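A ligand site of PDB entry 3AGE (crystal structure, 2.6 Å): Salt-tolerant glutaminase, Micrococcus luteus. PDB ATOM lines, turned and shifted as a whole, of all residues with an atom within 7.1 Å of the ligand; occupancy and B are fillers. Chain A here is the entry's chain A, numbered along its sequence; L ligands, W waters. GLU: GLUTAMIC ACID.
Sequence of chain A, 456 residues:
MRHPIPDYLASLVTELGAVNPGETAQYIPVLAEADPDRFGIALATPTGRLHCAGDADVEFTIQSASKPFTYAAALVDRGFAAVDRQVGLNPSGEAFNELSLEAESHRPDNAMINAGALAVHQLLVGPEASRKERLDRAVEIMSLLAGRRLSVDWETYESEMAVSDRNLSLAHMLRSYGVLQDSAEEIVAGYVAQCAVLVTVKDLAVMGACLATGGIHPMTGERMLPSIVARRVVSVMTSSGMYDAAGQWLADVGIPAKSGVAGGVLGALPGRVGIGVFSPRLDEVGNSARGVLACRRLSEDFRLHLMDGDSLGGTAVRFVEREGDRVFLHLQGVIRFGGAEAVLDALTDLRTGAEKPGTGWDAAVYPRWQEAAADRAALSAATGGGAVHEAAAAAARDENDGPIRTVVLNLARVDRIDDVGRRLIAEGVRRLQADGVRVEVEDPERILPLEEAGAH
OG of Ser 64 lies within hydrogen-bond range of O of Ser 259.
The side-chain amino group of Lys 258 sits at hydrogen-bond distance from the side-chain hydroxyl of Ser 64 (2.6 Å).
The side-chain amide nitrogen (NE2) of Gln 63 sits at hydrogen-bond distance from the backbone carbonyl oxygen (O) of Cys 195 (2.9 Å).
O of Gln 63 is in hydrogen-bond range of OG of Ser 66.
OH of Tyr 27 lies within hydrogen-bond range of OE1 of Glu 160.
OG of Ser 164 sits at hydrogen-bond distance from O of Glu 160 (2.6 Å).
OH of Tyr 191 is in hydrogen-bond range of OD1 of Asn 114, 3.3 Å away.
The backbone carbonyl oxygen of Tyr 191 is in hydrogen-bond range of the side-chain sulfur of Cys 195.
Water W2 lies within hydrogen-bond range of NZ of Lys 258 (2.7 Å), NZ of Lys 67 (3.0 Å), OE1 of the ligand (3.3 Å) and OG of Ser 64 (3.3 Å).
Water W3 lies within hydrogen-bond range of the backbone carbonyl oxygen (O) of Ser 259 and an oxygen (OE1) of the ligand.
N of Ser 64 lies close to OE2 of the ligand, 3.1 Å away.
The side-chain hydroxyl (OG) of Ser 64 sits at hydrogen-bond distance from an oxygen (OE2) of the ligand (2.5 Å).
The side-chain amide nitrogen of Asn 167 is in hydrogen-bond range of an oxygen (OXT) of the ligand (2.7 Å).
N of the ligand is in hydrogen-bond range of OE1 of Gln 63.
The side-chain carboxylate of Glu 160 lies within salt-bridge range of a nitrogen (N) of the ligand (2.8 Å).
N of Val 261 lies within hydrogen-bond range of OE2 of the ligand (3.1 Å).
An oxygen (OXT) of the ligand sits at hydrogen-bond distance from the side-chain hydroxyl of Tyr 191 (3.2 Å).
The side-chain amide nitrogen (ND2) of Asn 114 sits at hydrogen-bond distance from an oxygen (OXT) of the ligand, at 3.3 Å.
A nitrogen (N) of the ligand lies within hydrogen-bond range of the side-chain sulfur of Cys 195 (3.3 Å).
Merely in contact with the ligand: Gly 260 (3.2 Å) and Ser 259 (3.5 Å).
Hydrophobic or aromatic side chains that line the ligand: Tyr 191 and Val 261.
Ten residues have an atom within 4 Å of the ligand: Gln 63, Ser 64, Asn 114, Glu 160, Asn 167, Tyr 191, Cys 195, Ser 259, Gly 260 and Val 261.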
ATOM      1  N   TYR A  27     -24.038  -4.326 -21.643  1.00  0.00           N
ATOM      2  CA  TYR A  27     -24.854  -4.437 -20.427  1.00  0.00           C
ATOM      3  C   TYR A  27     -24.442  -3.545 -19.266  1.00  0.00           C
ATOM      4  O   TYR A  27     -25.278  -3.168 -18.447  1.00  0.00           O
ATOM      5  CB  TYR A  27     -24.928  -5.890 -19.986  1.00  0.00           C
ATOM      6  CG  TYR A  27     -23.833  -6.302 -19.044  1.00  0.00           C
ATOM      7  CD1 TYR A  27     -23.940  -6.060 -17.669  1.00  0.00           C
ATOM      8  CD2 TYR A  27     -22.698  -6.958 -19.505  1.00  0.00           C
ATOM      9  CE1 TYR A  27     -22.941  -6.470 -16.792  1.00  0.00           C
ATOM     10  CE2 TYR A  27     -21.702  -7.367 -18.641  1.00  0.00           C
ATOM     11  CZ  TYR A  27     -21.832  -7.125 -17.276  1.00  0.00           C
ATOM     12  OH  TYR A  27     -20.865  -7.556 -16.416  1.00  0.00           O
ATOM     13  N   LEU A  31     -17.798  -1.815 -18.705  1.00  0.00           N
ATOM     14  CA  LEU A  31     -17.250  -2.642 -19.769  1.00  0.00           C
ATOM     15  C   LEU A  31     -17.483  -2.068 -21.166  1.00  0.00           C
ATOM     16  O   LEU A  31     -16.677  -2.241 -22.078  1.00  0.00           O
ATOM     17  CB  LEU A  31     -17.795  -4.083 -19.695  1.00  0.00           C
ATOM     18  CG  LEU A  31     -17.422  -4.944 -18.489  1.00  0.00           C
ATOM     19  CD1 LEU A  31     -18.016  -6.332 -18.668  1.00  0.00           C
ATOM     20  CD2 LEU A  31     -15.920  -5.018 -18.372  1.00  0.00           C
ATOM     21  N   ILE A  62     -12.300 -11.236 -15.206  1.00  0.00           N
ATOM     22  CA  ILE A  62     -12.396 -12.581 -15.771  1.00  0.00           C
ATOM     23  C   ILE A  62     -13.812 -13.037 -16.110  1.00  0.00           C
ATOM     24  O   ILE A  62     -13.998 -13.964 -16.902  1.00  0.00           O
ATOM     25  CB  ILE A  62     -11.741 -13.605 -14.809  1.00  0.00           C
ATOM     26  CG1 ILE A  62     -11.599 -14.953 -15.508  1.00  0.00           C
ATOM     27  CG2 ILE A  62     -12.581 -13.770 -13.535  1.00  0.00           C
ATOM     28  CD1 ILE A  62     -10.730 -15.925 -14.771  1.00  0.00           C
ATOM     29  N   GLN A  63     -14.823 -12.399 -15.511  1.00  0.00           N
ATOM     30  CA  GLN A  63     -16.211 -12.763 -15.772  1.00  0.00           C
ATOM     31  C   GLN A  63     -16.435 -14.273 -15.765  1.00  0.00           C
ATOM     32  O   GLN A  63     -15.860 -14.984 -14.937  1.00  0.00           O
ATOM     33  CB  GLN A  63     -16.659 -12.175 -17.111  1.00  0.00           C
ATOM     34  CG  GLN A  63     -16.584 -10.651 -17.185  1.00  0.00           C
ATOM     35  CD  GLN A  63     -17.363  -9.968 -16.064  1.00  0.00           C
ATOM     36  OE1 GLN A  63     -18.526 -10.284 -15.831  1.00  0.00           O
ATOM     37  NE2 GLN A  63     -16.724  -9.015 -15.394  1.00  0.00           N
ATOM     38  N   SER A  64     -17.257 -14.766 -16.697  1.00  0.00           N
ATOM     39  CA  SER A  64     -17.576 -16.188 -16.759  1.00  0.00           C
ATOM     40  C   SER A  64     -16.383 -17.122 -16.880  1.00  0.00           C
ATOM     41  O   SER A  64     -16.536 -18.344 -16.752  1.00  0.00           O
ATOM     42  CB  SER A  64     -18.566 -16.477 -17.905  1.00  0.00           C
ATOM     43  OG  SER A  64     -17.928 -16.429 -19.161  1.00  0.00           O
ATOM     44  N   ALA A  65     -15.206 -16.580 -17.140  1.00  0.00           N
ATOM     45  CA  ALA A  65     -14.019 -17.430 -17.250  1.00  0.00           C
ATOM     46  C   ALA A  65     -13.651 -17.883 -15.840  1.00  0.00           C
ATOM     47  O   ALA A  65     -12.735 -18.676 -15.662  1.00  0.00           O
ATOM     48  CB  ALA A  65     -12.870 -16.675 -17.880  1.00  0.00           C
ATOM     49  N   SER A  66     -14.382 -17.371 -14.860  1.00  0.00           N
ATOM     50  CA  SER A  66     -14.160 -17.731 -13.465  1.00  0.00           C
ATOM     51  C   SER A  66     -14.909 -19.028 -13.130  1.00  0.00           C
ATOM     52  O   SER A  66     -14.582 -19.704 -12.154  1.00  0.00           O
ATOM     53  CB  SER A  66     -14.693 -16.640 -12.548  1.00  0.00           C
ATOM     54  OG  SER A  66     -16.097 -16.556 -12.635  1.00  0.00           O
ATOM     55  N   LYS A  67     -15.897 -19.368 -13.954  1.00  0.00           N
ATOM     56  CA  LYS A  67     -16.721 -20.547 -13.726  1.00  0.00           C
ATOM     57  C   LYS A  67     -16.008 -21.878 -13.582  1.00  0.00           C
ATOM     58  O   LYS A  67     -16.303 -22.651 -12.673  1.00  0.00           O
ATOM     59  CB  LYS A  67     -17.791 -20.621 -14.814  1.00  0.00           C
ATOM     60  CG  LYS A  67     -18.792 -19.459 -14.746  1.00  0.00           C
ATOM     61  CD  LYS A  67     -19.847 -19.562 -15.825  1.00  0.00           C
ATOM     62  CE  LYS A  67     -20.776 -18.369 -15.791  1.00  0.00           C
ATOM     63  NZ  LYS A  67     -21.772 -18.420 -16.907  1.00  0.00           N
ATOM     64  N   GLU A  94     -26.783 -20.675 -22.656  1.00  0.00           N
ATOM     65  CA  GLU A  94     -27.231 -19.826 -21.546  1.00  0.00           C
ATOM     66  C   GLU A  94     -28.745 -19.634 -21.434  1.00  0.00           C
ATOM     67  O   GLU A  94     -29.266 -19.432 -20.328  1.00  0.00           O
ATOM     68  CB  GLU A  94     -26.526 -18.466 -21.630  1.00  0.00           C
ATOM     69  CG  GLU A  94     -26.768 -17.536 -20.433  1.00  0.00           C
ATOM     70  CD  GLU A  94     -26.459 -18.190 -19.100  1.00  0.00           C
ATOM     71  OE1 GLU A  94     -25.396 -18.822 -18.980  1.00  0.00           O
ATOM     72  OE2 GLU A  94     -27.275 -18.064 -18.162  1.00  0.00           O
ATOM     73  N   MET A 112     -21.127 -24.334 -16.541  1.00  0.00           N
ATOM     74  CA  MET A 112     -20.704 -23.268 -17.443  1.00  0.00           C
ATOM     75  C   MET A 112     -21.740 -22.163 -17.658  1.00  0.00           C
ATOM     76  O   MET A 112     -21.392 -21.046 -18.026  1.00  0.00           O
ATOM     77  CB  MET A 112     -20.270 -23.864 -18.789  1.00  0.00           C
ATOM     78  CG  MET A 112     -19.064 -24.802 -18.665  1.00  0.00           C
ATOM     79  SD  MET A 112     -17.736 -24.137 -17.594  1.00  0.00           S
ATOM     80  CE  MET A 112     -17.052 -22.967 -18.667  1.00  0.00           C
ATOM     81  N   ASN A 114     -24.859 -19.553 -16.335  1.00  0.00           N
ATOM     82  CA  ASN A 114     -25.089 -18.751 -15.142  1.00  0.00           C
ATOM     83  C   ASN A 114     -25.815 -19.507 -14.032  1.00  0.00           C
ATOM     84  O   ASN A 114     -25.350 -19.552 -12.894  1.00  0.00           O
ATOM     85  CB  ASN A 114     -25.886 -17.501 -15.519  1.00  0.00           C
ATOM     86  CG  ASN A 114     -25.052 -16.481 -16.249  1.00  0.00           C
ATOM     87  OD1 ASN A 114     -23.953 -16.781 -16.718  1.00  0.00           O
ATOM     88  ND2 ASN A 114     -25.574 -15.262 -16.371  1.00  0.00           N
ATOM     89  N   GLU A 160     -22.314  -3.637 -12.438  1.00  0.00           N
ATOM     90  CA  GLU A 160     -23.124  -4.800 -12.803  1.00  0.00           C
ATOM     91  C   GLU A 160     -24.182  -5.167 -11.774  1.00  0.00           C
ATOM     92  O   GLU A 160     -25.250  -5.667 -12.140  1.00  0.00           O
ATOM     93  CB  GLU A 160     -22.217  -6.009 -13.089  1.00  0.00           C
ATOM     94  CG  GLU A 160     -22.944  -7.352 -13.196  1.00  0.00           C
ATOM     95  CD  GLU A 160     -22.053  -8.482 -13.710  1.00  0.00           C
ATOM     96  OE1 GLU A 160     -20.810  -8.349 -13.655  1.00  0.00           O
ATOM     97  OE2 GLU A 160     -22.598  -9.507 -14.169  1.00  0.00           O
ATOM     98  N   VAL A 163     -27.550  -3.791 -12.442  1.00  0.00           N
ATOM     99  CA  VAL A 163     -28.332  -4.343 -13.550  1.00  0.00           C
ATOM    100  C   VAL A 163     -28.210  -5.864 -13.608  1.00  0.00           C
ATOM    101  O   VAL A 163     -27.830  -6.431 -14.624  1.00  0.00           O
ATOM    102  CB  VAL A 163     -27.871  -3.755 -14.913  1.00  0.00           C
ATOM    103  CG1 VAL A 163     -28.143  -2.261 -14.941  1.00  0.00           C
ATOM    104  CG2 VAL A 163     -26.365  -4.017 -15.148  1.00  0.00           C
ATOM    105  N   SER A 164     -28.532  -6.524 -12.490  1.00  0.00           N
ATOM    106  CA  SER A 164     -28.469  -7.988 -12.418  1.00  0.00           C
ATOM    107  C   SER A 164     -29.835  -8.662 -12.335  1.00  0.00           C
ATOM    108  O   SER A 164     -29.960  -9.761 -11.782  1.00  0.00           O
ATOM    109  CB  SER A 164     -27.634  -8.411 -11.213  1.00  0.00           C
ATOM    110  OG  SER A 164     -26.295  -7.963 -11.332  1.00  0.00           O
ATOM    111  N   ARG A 166     -31.479 -10.283 -14.530  1.00  0.00           N
ATOM    112  CA  ARG A 166     -31.487 -11.620 -15.113  1.00  0.00           C
ATOM    113  C   ARG A 166     -30.907 -12.687 -14.184  1.00  0.00           C
ATOM    114  O   ARG A 166     -31.531 -13.731 -13.964  1.00  0.00           O
ATOM    115  CB  ARG A 166     -30.755 -11.661 -16.453  1.00  0.00           C
ATOM    116  CG  ARG A 166     -30.889 -13.039 -17.114  1.00  0.00           C
ATOM    117  CD  ARG A 166     -30.506 -13.051 -18.583  1.00  0.00           C
ATOM    118  NE  ARG A 166     -30.664 -14.380 -19.189  1.00  0.00           N
ATOM    119  CZ  ARG A 166     -29.835 -15.397 -18.989  1.00  0.00           C
ATOM    120  NH1 ARG A 166     -28.768 -15.252 -18.214  1.00  0.00           N
ATOM    121  NH2 ARG A 166     -30.064 -16.571 -19.568  1.00  0.00           N
ATOM    122  N   ASN A 167     -29.713 -12.433 -13.629  1.00  0.00           N
ATOM    123  CA  ASN A 167     -29.118 -13.409 -12.735  1.00  0.00           C
ATOM    124  C   ASN A 167     -29.927 -13.538 -11.443  1.00  0.00           C
ATOM    125  O   ASN A 167     -29.982 -14.604 -10.836  1.00  0.00           O
ATOM    126  CB  ASN A 167     -27.661 -13.052 -12.439  1.00  0.00           C
ATOM    127  CG  ASN A 167     -26.729 -13.483 -13.550  1.00  0.00           C
ATOM    128  OD1 ASN A 167     -26.820 -14.609 -14.045  1.00  0.00           O
ATOM    129  ND2 ASN A 167     -25.820 -12.603 -13.950  1.00  0.00           N
ATOM    130  N   TYR A 191     -21.424 -14.260  -6.971  1.00  0.00           N
ATOM    131  CA  TYR A 191     -21.079 -14.616  -8.341  1.00  0.00           C
ATOM    132  C   TYR A 191     -20.612 -13.401  -9.162  1.00  0.00           C
ATOM    133  O   TYR A 191     -19.734 -13.535 -10.013  1.00  0.00           O
ATOM    134  CB  TYR A 191     -22.289 -15.278  -9.007  1.00  0.00           C
ATOM    135  CG  TYR A 191     -22.205 -15.369 -10.512  1.00  0.00           C
ATOM    136  CD1 TYR A 191     -21.301 -16.233 -11.136  1.00  0.00           C
ATOM    137  CD2 TYR A 191     -22.991 -14.540 -11.314  1.00  0.00           C
ATOM    138  CE1 TYR A 191     -21.176 -16.258 -12.518  1.00  0.00           C
ATOM    139  CE2 TYR A 191     -22.876 -14.553 -12.692  1.00  0.00           C
ATOM    140  CZ  TYR A 191     -21.966 -15.420 -13.289  1.00  0.00           C
ATOM    141  OH  TYR A 191     -21.833 -15.396 -14.660  1.00  0.00           O
ATOM    142  N   VAL A 192     -21.181 -12.223  -8.898  1.00  0.00           N
ATOM    143  CA  VAL A 192     -20.795 -11.020  -9.621  1.00  0.00           C
ATOM    144  C   VAL A 192     -19.408 -10.538  -9.170  1.00  0.00           C
ATOM    145  O   VAL A 192     -18.622 -10.048  -9.976  1.00  0.00           O
ATOM    146  CB  VAL A 192     -21.831  -9.869  -9.437  1.00  0.00           C
ATOM    147  CG1 VAL A 192     -21.273  -8.550  -9.981  1.00  0.00           C
ATOM    148  CG2 VAL A 192     -23.126 -10.214 -10.163  1.00  0.00           C
ATOM    149  N   CYS A 195     -16.937 -12.575 -10.766  1.00  0.00           N
ATOM    150  CA  CYS A 195     -16.712 -12.143 -12.152  1.00  0.00           C
ATOM    151  C   CYS A 195     -15.872 -10.877 -12.220  1.00  0.00           C
ATOM    152  O   CYS A 195     -15.344 -10.539 -13.292  1.00  0.00           O
ATOM    153  CB  CYS A 195     -18.039 -11.892 -12.857  1.00  0.00           C
ATOM    154  SG  CYS A 195     -18.976 -13.377 -13.284  1.00  0.00           S
ATOM    155  N   ALA A 196     -15.770 -10.171 -11.099  1.00  0.00           N
ATOM    156  CA  ALA A 196     -15.017  -8.939 -11.063  1.00  0.00           C
ATOM    157  C   ALA A 196     -13.558  -9.158 -10.684  1.00  0.00           C
ATOM    158  O   ALA A 196     -12.797  -8.204 -10.544  1.00  0.00           O
ATOM    159  CB  ALA A 196     -15.663  -7.955 -10.096  1.00  0.00           C
ATOM    160  N   LYS A 258     -13.432 -21.089 -22.775  1.00  0.00           N
ATOM    161  CA  LYS A 258     -14.509 -20.305 -22.180  1.00  0.00           C
ATOM    162  C   LYS A 258     -14.195 -18.816 -22.349  1.00  0.00           C
ATOM    163  O   LYS A 258     -13.084 -18.368 -22.051  1.00  0.00           O
ATOM    164  CB  LYS A 258     -14.660 -20.624 -20.688  1.00  0.00           C
ATOM    165  CG  LYS A 258     -15.844 -19.936 -20.014  1.00  0.00           C
ATOM    166  CD  LYS A 258     -17.170 -20.508 -20.505  1.00  0.00           C
ATOM    167  CE  LYS A 258     -18.379 -19.747 -19.963  1.00  0.00           C
ATOM    168  NZ  LYS A 258     -18.581 -18.437 -20.650  1.00  0.00           N
ATOM    169  N   SER A 259     -15.163 -18.064 -22.835  1.00  0.00           N
ATOM    170  CA  SER A 259     -14.974 -16.636 -23.041  1.00  0.00           C
ATOM    171  C   SER A 259     -15.696 -15.813 -21.975  1.00  0.00           C
ATOM    172  O   SER A 259     -16.698 -16.273 -21.393  1.00  0.00           O
ATOM    173  CB  SER A 259     -15.497 -16.232 -24.429  1.00  0.00           C
ATOM    174  OG  SER A 259     -15.358 -14.835 -24.642  1.00  0.00           O
ATOM    175  N   GLY A 260     -15.170 -14.618 -21.723  1.00  0.00           N
ATOM    176  CA  GLY A 260     -15.763 -13.725 -20.743  1.00  0.00           C
ATOM    177  C   GLY A 260     -16.171 -12.441 -21.445  1.00  0.00           C
ATOM    178  O   GLY A 260     -15.437 -11.974 -22.315  1.00  0.00           O
ATOM    179  N   VAL A 261     -17.310 -11.864 -21.087  1.00  0.00           N
ATOM    180  CA  VAL A 261     -17.773 -10.647 -21.741  1.00  0.00           C
ATOM    181  C   VAL A 261     -16.863  -9.426 -21.603  1.00  0.00           C
ATOM    182  O   VAL A 261     -17.122  -8.382 -22.199  1.00  0.00           O
ATOM    183  CB  VAL A 261     -19.206 -10.251 -21.302  1.00  0.00           C
ATOM    184  CG1 VAL A 261     -20.191 -11.325 -21.726  1.00  0.00           C
ATOM    185  CG2 VAL A 261     -19.240 -10.030 -19.792  1.00  0.00           C
ATOM    186  N   ALA A 262     -15.806  -9.550 -20.807  1.00  0.00           N
ATOM    187  CA  ALA A 262     -14.869  -8.438 -20.637  1.00  0.00           C
ATOM    188  C   ALA A 262     -13.798  -8.562 -21.728  1.00  0.00           C
ATOM    189  O   ALA A 262     -12.922  -7.706 -21.860  1.00  0.00           O
ATOM    190  CB  ALA A 262     -14.230  -8.475 -19.261  1.00  0.00           C
ATOM    191  N   GLY A 264     -11.863 -11.602 -22.250  1.00  0.00           N
ATOM    192  CA  GLY A 264     -10.863 -12.632 -22.024  1.00  0.00           C
ATOM    193  C   GLY A 264     -11.325 -14.040 -22.360  1.00  0.00           C
ATOM    194  O   GLY A 264     -12.475 -14.403 -22.091  1.00  0.00           O
ATOM    195  N   GLY A 286     -21.633 -13.171 -28.324  1.00  0.00           N
ATOM    196  CA  GLY A 286     -21.132 -12.725 -27.040  1.00  0.00           C
ATOM    197  C   GLY A 286     -19.756 -13.190 -26.584  1.00  0.00           C
ATOM    198  O   GLY A 286     -19.421 -13.056 -25.402  1.00  0.00           O
ATOM    199  N   ASN A 287     -18.953 -13.743 -27.490  1.00  0.00           N
ATOM    200  CA  ASN A 287     -17.600 -14.161 -27.118  1.00  0.00           C
ATOM    201  C   ASN A 287     -16.614 -13.162 -27.725  1.00  0.00           C
ATOM    202  O   ASN A 287     -16.947 -12.429 -28.656  1.00  0.00           O
ATOM    203  CB  ASN A 287     -17.283 -15.569 -27.652  1.00  0.00           C
ATOM    204  CG  ASN A 287     -18.166 -16.649 -27.034  1.00  0.00           C
ATOM    205  OD1 ASN A 287     -18.364 -16.683 -25.825  1.00  0.00           O
ATOM    206  ND2 ASN A 287     -18.663 -17.540 -27.875  1.00  0.00           N
HETATM  207  N   GLU L   1     -20.961 -11.547 -15.247  1.00  0.00           N
HETATM  208  CA  GLU L   1     -21.696 -11.774 -16.517  1.00  0.00           C
HETATM  209  C   GLU L   1     -23.183 -11.973 -16.305  1.00  0.00           C
HETATM  210  O   GLU L   1     -23.941 -11.328 -17.056  1.00  0.00           O
HETATM  211  CB  GLU L   1     -21.143 -12.996 -17.257  1.00  0.00           C
HETATM  212  CG  GLU L   1     -20.044 -12.658 -18.204  1.00  0.00           C
HETATM  213  CD  GLU L   1     -19.775 -13.756 -19.208  1.00  0.00           C
HETATM  214  OE1 GLU L   1     -20.739 -14.281 -19.811  1.00  0.00           O
HETATM  215  OE2 GLU L   1     -18.597 -14.079 -19.412  1.00  0.00           O
HETATM  216  OXT GLU L   1     -23.585 -12.770 -15.427  1.00  0.00           O
HETATM  217  O   HOH W   1     -27.044 -12.169 -17.430  1.00  0.00           O
HETATM  218  O   HOH W   2     -20.979 -17.531 -19.696  1.00  0.00           O
HETATM  219  O   HOH W   3     -19.337 -15.507 -22.527  1.00  0.00           O
HETATM  220  O   HOH W   4     -23.453  -9.841 -19.659  1.00  0.00           O
